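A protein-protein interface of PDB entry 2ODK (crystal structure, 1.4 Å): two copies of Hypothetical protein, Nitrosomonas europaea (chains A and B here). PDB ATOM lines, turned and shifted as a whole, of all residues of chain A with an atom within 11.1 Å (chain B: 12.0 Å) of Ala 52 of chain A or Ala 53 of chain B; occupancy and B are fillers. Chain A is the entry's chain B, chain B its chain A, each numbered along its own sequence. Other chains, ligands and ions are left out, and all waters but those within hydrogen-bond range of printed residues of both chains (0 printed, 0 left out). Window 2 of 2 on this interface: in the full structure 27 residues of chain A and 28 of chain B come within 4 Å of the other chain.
The indole nitrogen (NE1) of Trp 46 of chain B lies close to the side-chain amide nitrogen (NE2) of Gln 50 of chain B (3.3 Å).
OE1 of Gln 50 of chain B is in hydrogen-bond range of NH1 of Arg 47 of chain B (3.2 Å).
The side-chain amide oxygen (OE1) of Gln 50 of chain A lies within hydrogen-bond range of the indole nitrogen (NE1) of Trp 46 of chain A, 3.2 Å away.
Among the printed residues, pairs that only touch across the chains: Leu 49 of chain A with Leu 49 of chain B, Trp 46 of chain A with Leu 49 of chain B, Ala 53 of chain A with Leu 49 of chain B, Trp 46 of chain A with Glu 45 of chain B, Glu 45 of chain A with Trp 46 of chain B, Ala 52 of chain A with Ala 53 of chain B, Leu 49 of chain A with Gln 50 of chain B, Ala 53 of chain A with Ala 52 of chain B and Gln 50 of chain A with Leu 49 of chain B.
Ile 43 of chain A touches none of the printed residues of chain B.
No residue of chain B comes within 4 Å of Ala 51 of chain A.
Ala 52 of chain A touches just one residue of chain B: Ala 53.
Gly 44 of chain B touches none of the printed residues of chain A.
Printed residues of chain A within 4 Å of Glu 45 of chain B: Trp 46.
Of the printed residues of chain A, Trp 46 of chain B touches Glu 45.
Ala 51 of chain B touches none of the printed residues of chain A.
Ala 52 of chain B touches just one residue of chain A: Ala 53.
Of the printed residues of chain A, Ala 53 of chain B touches Ala 52.
The nearest residue of chain B that does not touch Ala 52 of chain A is Ala 52 of chain B (4.1 Å).
The nearest printed residue of chain A that does not touch Ala 53 of chain B is Leu 49 of chain A (4.1 Å).
The nearest printed residue of chain B that does not touch Ala 53 of chain A is Ala 53 of chain B (4.2 Å).
Printed residues of chain A that touch a printed residue of chain B: Glu 45, Trp 46, Leu 49, Gln 50, Ala 52 and Ala 53.
Hydrophobic or aromatic side chains of chain A within 4 Å of the printed part of chain B: Trp 46, Leu 49, Ala 52 and Ala 53.
Among the printed residues, 9 pairs touch across the chains.
Glu 45 of chain A touches Trp 46 of chain B, and with the chains exchanged Trp 46 of chain A touches Glu 45 of chain B.
Leu 49 of chain A touches its own counterpart, Leu 49 of chain B.
Ala 52 of chain A touches Ala 53 of chain B, and with the chains exchanged Ala 53 of chain A touches Ala 52 of chain B.
Ala 53 of chain A touches Leu 49 of chain B, but with the chains exchanged Leu 49 of chain A does not touch Ala 53 of chain B (4.1 Å).
Positions printed for both chains: 44, 45, 46, 47, 48, 49, 50, 51, 52 and 53.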
ATOM      1  N   ILE A  43     -23.833  25.557 -24.837  1.00  0.00           N
ATOM      2  CA  ILE A  43     -24.828  25.570 -25.908  1.00  0.00           C
ATOM      3  C   ILE A  43     -24.325  24.911 -27.210  1.00  0.00           C
ATOM      4  O   ILE A  43     -25.078  24.198 -27.901  1.00  0.00           O
ATOM      5  CB  ILE A  43     -25.334  27.006 -26.143  1.00  0.00           C
ATOM      6  CG1 ILE A  43     -26.564  26.999 -27.051  1.00  0.00           C
ATOM      7  CG2 ILE A  43     -24.181  27.922 -26.644  1.00  0.00           C
ATOM      8  CD1 ILE A  43     -27.779  26.256 -26.454  1.00  0.00           C
ATOM      9  N   GLY A  44     -23.047  25.139 -27.535  1.00  0.00           N
ATOM     10  CA  GLY A  44     -22.493  24.547 -28.773  1.00  0.00           C
ATOM     11  C   GLY A  44     -22.476  23.031 -28.670  1.00  0.00           C
ATOM     12  O   GLY A  44     -22.911  22.323 -29.612  1.00  0.00           O
ATOM     13  N   GLU A  45     -21.999  22.533 -27.529  1.00  0.00           N
ATOM     14  CA  GLU A  45     -21.939  21.101 -27.270  1.00  0.00           C
ATOM     15  C   GLU A  45     -23.326  20.482 -27.342  1.00  0.00           C
ATOM     16  O   GLU A  45     -23.504  19.388 -27.934  1.00  0.00           O
ATOM     17  CB  GLU A  45     -21.266  20.832 -25.929  1.00  0.00           C
ATOM     18  CG  GLU A  45     -21.182  19.347 -25.577  1.00  0.00           C
ATOM     19  CD  GLU A  45     -20.363  19.074 -24.342  1.00  0.00           C
ATOM     20  OE1 GLU A  45     -19.544  19.939 -23.927  1.00  0.00           O
ATOM     21  OE2 GLU A  45     -20.507  17.963 -23.806  1.00  0.00           O
ATOM     22  N   TRP A  46     -24.315  21.155 -26.779  1.00  0.00           N
ATOM     23  CA  TRP A  46     -25.697  20.667 -26.874  1.00  0.00           C
ATOM     24  C   TRP A  46     -26.140  20.510 -28.330  1.00  0.00           C
ATOM     25  O   TRP A  46     -26.669  19.447 -28.734  1.00  0.00           O
ATOM     26  CB  TRP A  46     -26.626  21.633 -26.153  1.00  0.00           C
ATOM     27  CG  TRP A  46     -28.071  21.328 -26.278  1.00  0.00           C
ATOM     28  CD1 TRP A  46     -29.042  22.121 -26.850  1.00  0.00           C
ATOM     29  CD2 TRP A  46     -28.739  20.174 -25.766  1.00  0.00           C
ATOM     30  NE1 TRP A  46     -30.267  21.511 -26.736  1.00  0.00           N
ATOM     31  CE2 TRP A  46     -30.114  20.314 -26.093  1.00  0.00           C
ATOM     32  CE3 TRP A  46     -28.312  19.017 -25.104  1.00  0.00           C
ATOM     33  CZ2 TRP A  46     -31.072  19.352 -25.756  1.00  0.00           C
ATOM     34  CZ3 TRP A  46     -29.291  18.041 -24.768  1.00  0.00           C
ATOM     35  CH2 TRP A  46     -30.644  18.237 -25.093  1.00  0.00           C
ATOM     36  N   ARG A  47     -25.919  21.546 -29.128  1.00  0.00           N
ATOM     37  CA  ARG A  47     -26.323  21.520 -30.548  1.00  0.00           C
ATOM     38  C   ARG A  47     -25.600  20.394 -31.271  1.00  0.00           C
ATOM     39  O   ARG A  47     -26.208  19.650 -32.097  1.00  0.00           O
ATOM     40  CB  ARG A  47     -26.028  22.869 -31.232  1.00  0.00           C
ATOM     41  CG  ARG A  47     -26.648  24.120 -30.579  1.00  0.00           C
ATOM     42  CD  ARG A  47     -28.188  24.188 -30.607  1.00  0.00           C
ATOM     43  NE  ARG A  47     -28.652  25.564 -30.384  1.00  0.00           N
ATOM     44  CZ  ARG A  47     -29.836  25.909 -29.873  1.00  0.00           C
ATOM     45  NH1 ARG A  47     -30.706  24.974 -29.503  1.00  0.00           N
ATOM     46  NH2 ARG A  47     -30.141  27.200 -29.711  1.00  0.00           N
ATOM     47  N   ARG A  48     -24.317  20.242 -30.976  1.00  0.00           N
ATOM     48  CA  ARG A  48     -23.504  19.224 -31.648  1.00  0.00           C
ATOM     49  C   ARG A  48     -23.914  17.799 -31.275  1.00  0.00           C
ATOM     50  O   ARG A  48     -23.884  16.864 -32.111  1.00  0.00           O
ATOM     51  CB  ARG A  48     -22.038  19.430 -31.336  1.00  0.00           C
ATOM     52  CG  ARG A  48     -21.467  20.679 -32.044  1.00  0.00           C
ATOM     53  CD  ARG A  48     -19.975  20.775 -31.883  1.00  0.00           C
ATOM     54  NE  ARG A  48     -19.515  20.883 -30.489  1.00  0.00           N
ATOM     55  CZ  ARG A  48     -19.338  22.043 -29.836  1.00  0.00           C
ATOM     56  NH1 ARG A  48     -19.619  23.191 -30.429  1.00  0.00           N
ATOM     57  NH2 ARG A  48     -18.899  22.045 -28.578  1.00  0.00           N
ATOM     58  N   LEU A  49     -24.272  17.616 -30.011  1.00  0.00           N
ATOM     59  CA  LEU A  49     -24.739  16.310 -29.573  1.00  0.00           C
ATOM     60  C   LEU A  49     -26.055  15.966 -30.251  1.00  0.00           C
ATOM     61  O   LEU A  49     -26.264  14.786 -30.639  1.00  0.00           O
ATOM     62  CB  LEU A  49     -24.864  16.285 -28.047  1.00  0.00           C
ATOM     63  CG  LEU A  49     -24.012  15.286 -27.246  1.00  0.00           C
ATOM     64  CD1 LEU A  49     -24.871  14.108 -26.827  1.00  0.00           C
ATOM     65  CD2 LEU A  49     -22.755  14.790 -27.962  1.00  0.00           C
ATOM     66  N   GLN A  50     -26.943  16.949 -30.388  1.00  0.00           N
ATOM     67  CA  GLN A  50     -28.219  16.685 -31.024  1.00  0.00           C
ATOM     68  C   GLN A  50     -27.990  16.232 -32.468  1.00  0.00           C
ATOM     69  O   GLN A  50     -28.672  15.281 -32.928  1.00  0.00           O
ATOM     70  CB  GLN A  50     -29.165  17.875 -30.920  1.00  0.00           C
ATOM     71  CG  GLN A  50     -29.726  18.075 -29.503  1.00  0.00           C
ATOM     72  CD  GLN A  50     -30.695  19.229 -29.423  1.00  0.00           C
ATOM     73  OE1 GLN A  50     -30.336  20.377 -29.693  1.00  0.00           O
ATOM     74  NE2 GLN A  50     -31.935  18.937 -29.045  1.00  0.00           N
ATOM     75  N   ALA A  51     -27.021  16.845 -33.147  1.00  0.00           N
ATOM     76  CA  ALA A  51     -26.664  16.475 -34.544  1.00  0.00           C
ATOM     77  C   ALA A  51     -26.023  15.080 -34.603  1.00  0.00           C
ATOM     78  O   ALA A  51     -26.332  14.276 -35.504  1.00  0.00           O
ATOM     79  CB  ALA A  51     -25.731  17.537 -35.162  1.00  0.00           C
ATOM     80  N   ALA A  52     -25.142  14.782 -33.650  1.00  0.00           N
ATOM     81  CA  ALA A  52     -24.481  13.470 -33.549  1.00  0.00           C
ATOM     82  C   ALA A  52     -25.437  12.313 -33.161  1.00  0.00           C
ATOM     83  O   ALA A  52     -25.158  11.138 -33.469  1.00  0.00           O
ATOM     84  CB  ALA A  52     -23.335  13.533 -32.573  1.00  0.00           C
ATOM     85  N   ALA A  53     -26.530  12.624 -32.471  1.00  0.00           N
ATOM     86  CA  ALA A  53     -27.488  11.572 -32.094  1.00  0.00           C
ATOM     87  C   ALA A  53     -28.415  11.255 -33.271  1.00  0.00           C
ATOM     88  O   ALA A  53     -28.895  12.164 -33.966  1.00  0.00           O
ATOM     89  CB  ALA A  53     -28.286  11.972 -30.857  1.00  0.00           C
ATOM     90  N   GLY B  44     -31.987  12.673 -17.633  1.00  0.00           N
ATOM     91  CA  GLY B  44     -32.294  11.438 -18.394  1.00  0.00           C
ATOM     92  C   GLY B  44     -32.210  11.691 -19.889  1.00  0.00           C
ATOM     93  O   GLY B  44     -31.741  10.828 -20.668  1.00  0.00           O
ATOM     94  N   GLU B  45     -32.660  12.883 -20.302  1.00  0.00           N
ATOM     95  CA  GLU B  45     -32.605  13.229 -21.716  1.00  0.00           C
ATOM     96  C   GLU B  45     -31.146  13.340 -22.176  1.00  0.00           C
ATOM     97  O   GLU B  45     -30.789  12.844 -23.262  1.00  0.00           O
ATOM     98  CB  GLU B  45     -33.330  14.560 -21.942  1.00  0.00           C
ATOM     99  CG  GLU B  45     -33.269  15.049 -23.375  1.00  0.00           C
ATOM    100  CD  GLU B  45     -34.166  16.260 -23.637  1.00  0.00           C
ATOM    101  OE1 GLU B  45     -35.118  16.483 -22.864  1.00  0.00           O
ATOM    102  OE2 GLU B  45     -33.932  16.985 -24.643  1.00  0.00           O
ATOM    103  N   TRP B  46     -30.294  13.985 -21.348  1.00  0.00           N
ATOM    104  CA  TRP B  46     -28.885  14.050 -21.656  1.00  0.00           C
ATOM    105  C   TRP B  46     -28.247  12.655 -21.766  1.00  0.00           C
ATOM    106  O   TRP B  46     -27.492  12.373 -22.728  1.00  0.00           O
ATOM    107  CB  TRP B  46     -28.206  14.857 -20.535  1.00  0.00           C
ATOM    108  CG  TRP B  46     -26.706  14.836 -20.513  1.00  0.00           C
ATOM    109  CD1 TRP B  46     -25.875  14.227 -19.577  1.00  0.00           C
ATOM    110  CD2 TRP B  46     -25.887  15.473 -21.433  1.00  0.00           C
ATOM    111  NE1 TRP B  46     -24.572  14.468 -19.903  1.00  0.00           N
ATOM    112  CE2 TRP B  46     -24.540  15.248 -21.028  1.00  0.00           C
ATOM    113  CE3 TRP B  46     -26.137  16.255 -22.532  1.00  0.00           C
ATOM    114  CZ2 TRP B  46     -23.461  15.742 -21.723  1.00  0.00           C
ATOM    115  CZ3 TRP B  46     -25.011  16.768 -23.248  1.00  0.00           C
ATOM    116  CH2 TRP B  46     -23.718  16.510 -22.829  1.00  0.00           C
ATOM    117  N   ARG B  47     -28.536  11.775 -20.800  1.00  0.00           N
ATOM    118  CA  ARG B  47     -27.919  10.435 -20.836  1.00  0.00           C
ATOM    119  C   ARG B  47     -28.304   9.708 -22.129  1.00  0.00           C
ATOM    120  O   ARG B  47     -27.473   9.056 -22.754  1.00  0.00           O
ATOM    121  CB  ARG B  47     -28.366   9.574 -19.657  1.00  0.00           C
ATOM    122  CG  ARG B  47     -27.985  10.115 -18.272  1.00  0.00           C
ATOM    123  CD  ARG B  47     -26.486  10.263 -18.120  1.00  0.00           C
ATOM    124  NE  ARG B  47     -26.117  10.660 -16.766  1.00  0.00           N
ATOM    125  CZ  ARG B  47     -24.866  10.985 -16.432  1.00  0.00           C
ATOM    126  NH1 ARG B  47     -23.902  10.881 -17.354  1.00  0.00           N
ATOM    127  NH2 ARG B  47     -24.564  11.331 -15.193  1.00  0.00           N
ATOM    128  N   ARG B  48     -29.575   9.838 -22.520  1.00  0.00           N
ATOM    129  CA  ARG B  48     -29.997   9.133 -23.737  1.00  0.00           C
ATOM    130  C   ARG B  48     -29.350   9.714 -24.984  1.00  0.00           C
ATOM    131  O   ARG B  48     -28.989   8.975 -25.901  1.00  0.00           O
ATOM    132  CB  ARG B  48     -31.518   9.094 -23.851  1.00  0.00           C
ATOM    133  CG  ARG B  48     -32.110   8.175 -22.751  1.00  0.00           C
ATOM    134  CD  ARG B  48     -33.611   8.018 -22.953  1.00  0.00           C
ATOM    135  NE  ARG B  48     -34.361   9.256 -22.799  1.00  0.00           N
ATOM    136  CZ  ARG B  48     -34.825   9.734 -21.644  1.00  0.00           C
ATOM    137  NH1 ARG B  48     -34.627   9.072 -20.483  1.00  0.00           N
ATOM    138  NH2 ARG B  48     -35.480  10.897 -21.612  1.00  0.00           N
ATOM    139  N   LEU B  49     -29.170  11.027 -24.990  1.00  0.00           N
ATOM    140  CA  LEU B  49     -28.468  11.709 -26.088  1.00  0.00           C
ATOM    141  C   LEU B  49     -27.034  11.193 -26.195  1.00  0.00           C
ATOM    142  O   LEU B  49     -26.507  10.922 -27.296  1.00  0.00           O
ATOM    143  CB  LEU B  49     -28.425  13.229 -25.804  1.00  0.00           C
ATOM    144  CG  LEU B  49     -27.749  14.146 -26.833  1.00  0.00           C
ATOM    145  CD1 LEU B  49     -28.416  13.920 -28.168  1.00  0.00           C
ATOM    146  CD2 LEU B  49     -27.922  15.588 -26.438  1.00  0.00           C
ATOM    147  N   GLN B  50     -26.372  11.100 -25.034  1.00  0.00           N
ATOM    148  CA  GLN B  50     -24.985  10.577 -24.933  1.00  0.00           C
ATOM    149  C   GLN B  50     -24.905   9.160 -25.506  1.00  0.00           C
ATOM    150  O   GLN B  50     -23.971   8.827 -26.261  1.00  0.00           O
ATOM    151  CB  GLN B  50     -24.479  10.559 -23.466  1.00  0.00           C
ATOM    152  CG  GLN B  50     -24.108  11.927 -22.796  1.00  0.00           C
ATOM    153  CD  GLN B  50     -23.576  11.752 -21.354  1.00  0.00           C
ATOM    154  OE1 GLN B  50     -24.227  11.142 -20.497  1.00  0.00           O
ATOM    155  NE2 GLN B  50     -22.377  12.262 -21.093  1.00  0.00           N
ATOM    156  N   ALA B  51     -25.870   8.326 -25.130  1.00  0.00           N
ATOM    157  CA  ALA B  51     -25.853   6.926 -25.563  1.00  0.00           C
ATOM    158  C   ALA B  51     -26.064   6.841 -27.068  1.00  0.00           C
ATOM    159  O   ALA B  51     -25.498   5.926 -27.706  1.00  0.00           O
ATOM    160  CB  ALA B  51     -26.902   6.109 -24.817  1.00  0.00           C
ATOM    161  N   ALA B  52     -26.836   7.762 -27.640  1.00  0.00           N
ATOM    162  CA  ALA B  52     -27.184   7.684 -29.081  1.00  0.00           C
ATOM    163  C   ALA B  52     -26.075   8.268 -29.934  1.00  0.00           C
ATOM    164  O   ALA B  52     -25.943   7.906 -31.109  1.00  0.00           O
ATOM    165  CB  ALA B  52     -28.480   8.403 -29.373  1.00  0.00           C
ATOM    166  N   ALA B  53     -25.310   9.189 -29.360  1.00  0.00           N
ATOM    167  CA  ALA B  53     -24.171   9.819 -30.046  1.00  0.00           C
ATOM    168  C   ALA B  53     -22.938   8.976 -29.818  1.00  0.00           C
ATOM    169  O   ALA B  53     -22.502   8.273 -30.719  1.00  0.00           O
ATOM    170  CB  ALA B  53     -23.944  11.209 -29.526  1.00  0.00           C
